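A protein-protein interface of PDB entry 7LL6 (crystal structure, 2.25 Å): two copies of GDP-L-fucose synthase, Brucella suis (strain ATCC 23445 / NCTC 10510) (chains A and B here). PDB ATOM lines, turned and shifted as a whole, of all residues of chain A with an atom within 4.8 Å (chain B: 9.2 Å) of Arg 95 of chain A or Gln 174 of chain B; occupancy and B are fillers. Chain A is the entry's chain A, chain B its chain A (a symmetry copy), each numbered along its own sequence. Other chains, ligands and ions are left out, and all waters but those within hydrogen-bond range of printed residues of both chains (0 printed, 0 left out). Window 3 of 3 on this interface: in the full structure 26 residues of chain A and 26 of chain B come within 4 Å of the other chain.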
ATOM      1  N   LEU A  91       7.007  15.094  13.923  1.00  0.00           N
ATOM      2  CA  LEU A  91       7.863  14.020  13.435  1.00  0.00           C
ATOM      3  C   LEU A  91       7.362  13.469  12.108  1.00  0.00           C
ATOM      4  O   LEU A  91       8.164  13.188  11.213  1.00  0.00           O
ATOM      5  CB  LEU A  91       7.965  12.898  14.475  1.00  0.00           C
ATOM      6  CG  LEU A  91       8.509  13.282  15.858  1.00  0.00           C
ATOM      7  CD1 LEU A  91       8.268  12.160  16.890  1.00  0.00           C
ATOM      8  CD2 LEU A  91       9.994  13.616  15.748  1.00  0.00           C
ATOM      9  N   ALA A  92       6.044  13.302  11.952  1.00  0.00           N
ATOM     10  CA  ALA A  92       5.537  12.832  10.662  1.00  0.00           C
ATOM     11  C   ALA A  92       5.802  13.857   9.556  1.00  0.00           C
ATOM     12  O   ALA A  92       6.308  13.510   8.483  1.00  0.00           O
ATOM     13  CB  ALA A  92       4.045  12.506  10.757  1.00  0.00           C
ATOM     14  N   ASN A  93       5.461  15.124   9.803  1.00  0.00           N
ATOM     15  CA  ASN A  93       5.684  16.163   8.800  1.00  0.00           C
ATOM     16  C   ASN A  93       7.144  16.222   8.385  1.00  0.00           C
ATOM     17  O   ASN A  93       7.453  16.361   7.197  1.00  0.00           O
ATOM     18  CB  ASN A  93       5.238  17.522   9.336  1.00  0.00           C
ATOM     19  CG  ASN A  93       3.779  17.791   9.099  1.00  0.00           C
ATOM     20  OD1 ASN A  93       3.398  18.265   8.026  1.00  0.00           O
ATOM     21  ND2 ASN A  93       2.944  17.504  10.097  1.00  0.00           N
ATOM     22  N   SER A  94       8.061  16.099   9.342  1.00  0.00           N
ATOM     23  CA  SER A  94       9.465  16.253   8.989  1.00  0.00           C
ATOM     24  C   SER A  94      10.025  15.019   8.300  1.00  0.00           C
ATOM     25  O   SER A  94      10.958  15.142   7.501  1.00  0.00           O
ATOM     26  CB  SER A  94      10.285  16.595  10.232  1.00  0.00           C
ATOM     27  OG  SER A  94      10.566  15.439  10.991  1.00  0.00           O
ATOM     28  N   ARG A  95       9.478  13.829   8.562  1.00  0.00           N
ATOM     29  CA  ARG A  95      10.013  12.630   7.924  1.00  0.00           C
ATOM     30  C   ARG A  95       9.272  12.223   6.650  1.00  0.00           C
ATOM     31  O   ARG A  95       9.804  11.416   5.880  1.00  0.00           O
ATOM     32  CB  ARG A  95      10.007  11.446   8.906  1.00  0.00           C
ATOM     33  N   PHE A  96       8.057  12.713   6.418  1.00  0.00           N
ATOM     34  CA  PHE A  96       7.288  12.348   5.225  1.00  0.00           C
ATOM     35  C   PHE A  96       6.819  13.602   4.487  1.00  0.00           C
ATOM     36  O   PHE A  96       5.638  13.751   4.168  1.00  0.00           O
ATOM     37  CB  PHE A  96       6.094  11.460   5.581  1.00  0.00           C
ATOM     38  CG  PHE A  96       6.450  10.248   6.416  1.00  0.00           C
ATOM     39  CD1 PHE A  96       7.317   9.285   5.935  1.00  0.00           C
ATOM     40  CD2 PHE A  96       5.903  10.069   7.679  1.00  0.00           C
ATOM     41  CE1 PHE A  96       7.640   8.177   6.701  1.00  0.00           C
ATOM     42  CE2 PHE A  96       6.234   8.952   8.450  1.00  0.00           C
ATOM     43  CZ  PHE A  96       7.093   8.019   7.956  1.00  0.00           C
ATOM     44  N   PRO A  97       7.732  14.532   4.185  1.00  0.00           N
ATOM     45  CA  PRO A  97       7.280  15.785   3.566  1.00  0.00           C
ATOM     46  C   PRO A  97       6.584  15.557   2.234  1.00  0.00           C
ATOM     47  O   PRO A  97       5.523  16.143   2.004  1.00  0.00           O
ATOM     48  CB  PRO A  97       8.580  16.584   3.431  1.00  0.00           C
ATOM     49  CG  PRO A  97       9.624  15.538   3.244  1.00  0.00           C
ATOM     50  CD  PRO A  97       9.196  14.372   4.099  1.00  0.00           C
ATOM     51  N   ALA A  98       7.115  14.670   1.378  1.00  0.00           N
ATOM     52  CA  ALA A  98       6.494  14.431   0.072  1.00  0.00           C
ATOM     53  C   ALA A  98       5.050  13.947   0.205  1.00  0.00           C
ATOM     54  O   ALA A  98       4.163  14.363  -0.559  1.00  0.00           O
ATOM     55  CB  ALA A  98       7.328  13.419  -0.726  1.00  0.00           C
ATOM     56  N   ASP A  99       4.783  13.081   1.175  1.00  0.00           N
ATOM     57  CA  ASP A  99       3.406  12.633   1.367  1.00  0.00           C
ATOM     58  C   ASP A  99       2.517  13.749   1.878  1.00  0.00           C
ATOM     59  O   ASP A  99       1.351  13.871   1.463  1.00  0.00           O
ATOM     60  CB  ASP A  99       3.393  11.454   2.339  1.00  0.00           C
ATOM     61  CG  ASP A  99       4.036  10.253   1.738  1.00  0.00           C
ATOM     62  OD1 ASP A  99       3.698   9.965   0.569  1.00  0.00           O
ATOM     63  OD2 ASP A  99       4.894   9.629   2.394  1.00  0.00           O
ATOM     64  N   HIS B 116       8.377   9.925  -9.464  1.00  0.00           N
ATOM     65  CA  HIS B 116       8.720   9.259  -8.212  1.00  0.00           C
ATOM     66  C   HIS B 116       8.191   7.834  -8.175  1.00  0.00           C
ATOM     67  O   HIS B 116       8.873   6.936  -7.671  1.00  0.00           O
ATOM     68  CB  HIS B 116       8.191  10.016  -6.991  1.00  0.00           C
ATOM     69  CG  HIS B 116       8.179   9.161  -5.766  1.00  0.00           C
ATOM     70  ND1 HIS B 116       9.332   8.814  -5.096  1.00  0.00           N
ATOM     71  CD2 HIS B 116       7.172   8.484  -5.161  1.00  0.00           C
ATOM     72  CE1 HIS B 116       9.033   7.987  -4.108  1.00  0.00           C
ATOM     73  NE2 HIS B 116       7.727   7.779  -4.119  1.00  0.00           N
ATOM     74  N   LYS B 166       8.884  22.940  -4.552  1.00  0.00           N
ATOM     75  CA  LYS B 166       8.890  22.354  -3.204  1.00  0.00           C
ATOM     76  C   LYS B 166       8.463  20.894  -3.226  1.00  0.00           C
ATOM     77  O   LYS B 166       8.958  20.089  -2.430  1.00  0.00           O
ATOM     78  CB  LYS B 166       7.981  23.167  -2.287  1.00  0.00           C
ATOM     79  CG  LYS B 166       8.584  24.535  -2.001  1.00  0.00           C
ATOM     80  CD  LYS B 166       9.731  24.341  -1.046  1.00  0.00           C
ATOM     81  CE  LYS B 166      10.442  25.628  -0.665  1.00  0.00           C
ATOM     82  NZ  LYS B 166      11.592  25.315   0.275  1.00  0.00           N
ATOM     83  N   TYR B 167       7.588  20.522  -4.153  1.00  0.00           N
ATOM     84  CA  TYR B 167       7.250  19.114  -4.262  1.00  0.00           C
ATOM     85  C   TYR B 167       8.445  18.315  -4.770  1.00  0.00           C
ATOM     86  O   TYR B 167       8.732  17.227  -4.251  1.00  0.00           O
ATOM     87  CB  TYR B 167       6.010  18.931  -5.142  1.00  0.00           C
ATOM     88  CG  TYR B 167       5.592  17.479  -5.302  1.00  0.00           C
ATOM     89  CD1 TYR B 167       5.697  16.568  -4.237  1.00  0.00           C
ATOM     90  CD2 TYR B 167       5.089  17.025  -6.507  1.00  0.00           C
ATOM     91  CE1 TYR B 167       5.313  15.242  -4.381  1.00  0.00           C
ATOM     92  CE2 TYR B 167       4.692  15.705  -6.663  1.00  0.00           C
ATOM     93  CZ  TYR B 167       4.822  14.811  -5.612  1.00  0.00           C
ATOM     94  OH  TYR B 167       4.429  13.493  -5.769  1.00  0.00           O
ATOM     95  N   ALA B 168       9.196  18.853  -5.739  1.00  0.00           N
ATOM     96  CA  ALA B 168      10.448  18.192  -6.105  1.00  0.00           C
ATOM     97  C   ALA B 168      11.395  18.110  -4.914  1.00  0.00           C
ATOM     98  O   ALA B 168      12.005  17.060  -4.668  1.00  0.00           O
ATOM     99  CB  ALA B 168      11.134  18.919  -7.267  1.00  0.00           C
ATOM    100  N   GLN B 169      11.538  19.208  -4.165  1.00  0.00           N
ATOM    101  CA  GLN B 169      12.430  19.169  -3.005  1.00  0.00           C
ATOM    102  C   GLN B 169      12.010  18.086  -2.019  1.00  0.00           C
ATOM    103  O   GLN B 169      12.855  17.379  -1.463  1.00  0.00           O
ATOM    104  CB  GLN B 169      12.446  20.514  -2.286  1.00  0.00           C
ATOM    105  CG  GLN B 169      13.355  21.570  -2.852  1.00  0.00           C
ATOM    106  CD  GLN B 169      13.329  22.825  -1.998  1.00  0.00           C
ATOM    107  OE1 GLN B 169      12.679  22.863  -0.941  1.00  0.00           O
ATOM    108  NE2 GLN B 169      14.013  23.866  -2.454  1.00  0.00           N
ATOM    109  N   SER B 170      10.707  17.960  -1.765  1.00  0.00           N
ATOM    110  CA  SER B 170      10.267  17.009  -0.752  1.00  0.00           C
ATOM    111  C   SER B 170      10.536  15.576  -1.192  1.00  0.00           C
ATOM    112  O   SER B 170      10.886  14.728  -0.361  1.00  0.00           O
ATOM    113  CB  SER B 170       8.786  17.240  -0.430  1.00  0.00           C
ATOM    114  OG  SER B 170       7.961  16.857  -1.530  1.00  0.00           O
ATOM    115  N   CYS B 171      10.440  15.296  -2.497  1.00  0.00           N
ATOM    116  CA  CYS B 171      10.779  13.958  -2.980  1.00  0.00           C
ATOM    117  C   CYS B 171      12.259  13.655  -2.817  1.00  0.00           C
ATOM    118  O   CYS B 171      12.629  12.532  -2.466  1.00  0.00           O
ATOM    119  CB  CYS B 171      10.391  13.805  -4.440  1.00  0.00           C
ATOM    120  SG  CYS B 171       8.643  13.737  -4.712  1.00  0.00           S
ATOM    121  N   ALA B 172      13.123  14.627  -3.102  1.00  0.00           N
ATOM    122  CA  ALA B 172      14.545  14.424  -2.846  1.00  0.00           C
ATOM    123  C   ALA B 172      14.794  14.227  -1.359  1.00  0.00           C
ATOM    124  O   ALA B 172      15.537  13.325  -0.962  1.00  0.00           O
ATOM    125  CB  ALA B 172      15.362  15.600  -3.411  1.00  0.00           C
ATOM    126  N   ARG B 173      14.125  15.013  -0.519  1.00  0.00           N
ATOM    127  CA  ARG B 173      14.292  14.877   0.927  1.00  0.00           C
ATOM    128  C   ARG B 173      13.836  13.517   1.441  1.00  0.00           C
ATOM    129  O   ARG B 173      14.554  12.853   2.196  1.00  0.00           O
ATOM    130  CB  ARG B 173      13.507  15.968   1.647  1.00  0.00           C
ATOM    131  CG  ARG B 173      14.340  17.154   1.937  1.00  0.00           C
ATOM    132  CD  ARG B 173      13.507  18.306   2.396  1.00  0.00           C
ATOM    133  NE  ARG B 173      14.304  19.507   2.218  1.00  0.00           N
ATOM    134  CZ  ARG B 173      13.805  20.700   1.949  1.00  0.00           C
ATOM    135  NH1 ARG B 173      12.502  20.889   1.835  1.00  0.00           N
ATOM    136  NH2 ARG B 173      14.636  21.727   1.785  1.00  0.00           N
ATOM    137  N   GLN B 174      12.611  13.124   1.111  1.00  0.00           N
ATOM    138  CA  GLN B 174      12.028  11.946   1.738  1.00  0.00           C
ATOM    139  C   GLN B 174      12.579  10.660   1.143  1.00  0.00           C
ATOM    140  O   GLN B 174      12.817   9.694   1.874  1.00  0.00           O
ATOM    141  CB  GLN B 174      10.506  11.982   1.605  1.00  0.00           C
ATOM    142  CG  GLN B 174       9.832  10.768   2.232  1.00  0.00           C
ATOM    143  CD  GLN B 174       8.321  10.890   2.275  1.00  0.00           C
ATOM    144  OE1 GLN B 174       7.770  11.990   2.165  1.00  0.00           O
ATOM    145  NE2 GLN B 174       7.639   9.756   2.459  1.00  0.00           N
ATOM    146  N   PHE B 175      12.799  10.628  -0.172  1.00  0.00           N
ATOM    147  CA  PHE B 175      13.189   9.406  -0.860  1.00  0.00           C
ATOM    148  C   PHE B 175      14.587   9.430  -1.449  1.00  0.00           C
ATOM    149  O   PHE B 175      15.092   8.369  -1.826  1.00  0.00           O
ATOM    150  CB  PHE B 175      12.219   9.101  -2.012  1.00  0.00           C
ATOM    151  CG  PHE B 175      10.783   9.198  -1.631  1.00  0.00           C
ATOM    152  CD1 PHE B 175      10.200   8.241  -0.803  1.00  0.00           C
ATOM    153  CD2 PHE B 175      10.003  10.230  -2.114  1.00  0.00           C
ATOM    154  CE1 PHE B 175       8.860   8.329  -0.458  1.00  0.00           C
ATOM    155  CE2 PHE B 175       8.667  10.318  -1.784  1.00  0.00           C
ATOM    156  CZ  PHE B 175       8.096   9.366  -0.947  1.00  0.00           C
ATOM    157  N   GLY B 176      15.220  10.595  -1.566  1.00  0.00           N
ATOM    158  CA  GLY B 176      16.473  10.618  -2.297  1.00  0.00           C
ATOM    159  C   GLY B 176      16.284  10.659  -3.790  1.00  0.00           C
ATOM    160  O   GLY B 176      17.223  10.379  -4.532  1.00  0.00           O
ATOM    161  N   ASP B 177      15.081  10.982  -4.258  1.00  0.00           N
ATOM    162  CA  ASP B 177      14.876  11.209  -5.681  1.00  0.00           C
ATOM    163  C   ASP B 177      15.757  12.370  -6.137  1.00  0.00           C
ATOM    164  O   ASP B 177      15.794  13.420  -5.495  1.00  0.00           O
ATOM    165  CB  ASP B 177      13.398  11.508  -5.952  1.00  0.00           C
ATOM    166  CG  ASP B 177      12.499  10.286  -5.754  1.00  0.00           C
ATOM    167  OD1 ASP B 177      12.948   9.158  -6.073  1.00  0.00           O
ATOM    168  OD2 ASP B 177      11.340  10.462  -5.289  1.00  0.00           O
ATOM    169  N   ILE B 252      19.704  19.842  -3.382  1.00  0.00           N
ATOM    170  CA  ILE B 252      18.258  19.869  -3.273  1.00  0.00           C
ATOM    171  C   ILE B 252      17.711  21.250  -3.588  1.00  0.00           C
ATOM    172  O   ILE B 252      16.685  21.371  -4.258  1.00  0.00           O
ATOM    173  CB  ILE B 252      17.853  19.407  -1.854  1.00  0.00           C
ATOM    174  CG1 ILE B 252      18.247  17.939  -1.634  1.00  0.00           C
ATOM    175  CG2 ILE B 252      16.364  19.655  -1.582  1.00  0.00           C
ATOM    176  CD1 ILE B 252      18.003  17.463  -0.240  1.00  0.00           C
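OE1 of Gln 174 of chain B is in hydrogen-bond range of N of Ala 98 of chain A.
OD2 of Asp 99 of chain A lies within hydrogen-bond range of NE2 of Gln 174 of chain B (2.7 Å).
OE1 of Gln 174 of chain B sits close to N of Pro 97 of chain A.
OE1 of Gln 174 of chain B sits close to O of Phe 96 of chain A.
The backbone carbonyl oxygen of Tyr 167 of chain B is in hydrogen-bond range of the side-chain hydroxyl of Ser 170 of chain B (2.9 Å).
Among the printed residues, merely in contact across the chains: Arg 95 of chain A with Gln 174 of chain B (3.7 Å), Pro 97 of chain A with Ser 170 of chain B (3.8 Å), Ala 98 of chain A with Ser 170 of chain B (3.3 Å) and Ala 98 of chain A with Phe 175 of chain B (3.5 Å).
Of chain B, only Gln 174 comes within 4 Å of Arg 95 of chain A.
Gln 174 of chain B touches five residues of chain A.
No residue of chain B comes within 4 Å of Ser 94 of chain A.
Pro 97 of chain A touches just these residues of chain B: Ser 170 (3.8 Å) and Gln 174 (3.2 Å).
Ala 98 of chain A touches just these residues of chain B: Ser 170 (3.3 Å), Gln 174 (2.9 Å) and Phe 175 (3.5 Å).
Of the printed residues of chain A, Ser 170 of chain B touches Pro 97 and Ala 98.
Printed residues of chain B within 4 Å of Asp 99 of chain A: Gln 174 (2.7 Å).
Printed residues of chain A within 4 Å of Phe 175 of chain B: Ala 98 (3.5 Å).
Ala 172 of chain B touches none of the printed residues of chain A.
Ile 252 of chain B touches none of the printed residues of chain A.
The nearest residue of chain B that does not touch Arg 95 of chain A is Arg 173 of chain B (6.2 Å).
The nearest printed residue of chain A that does not touch Ser 170 of chain B is Asp 99 of chain A (5.6 Å).
Hydrophobic or aromatic side chains of chain A within 4 Å of the printed part of chain B: Phe 96, Pro 97 and Ala 98.
Printed residues of chain B that touch a printed residue of chain A: Ser 170, Gln 174 and Phe 175.
Among the printed residues, 8 pairs touch across the chains.
Among the printed residues, no Asp or Glu carboxylate lies within 4 Å of a Lys or Arg side-chain nitrogen of the other chain.
No position is printed for both chains.
Of the 8 pairs that touch across the chains among the printed residues, none has its exchanged pair printed and touching as well.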
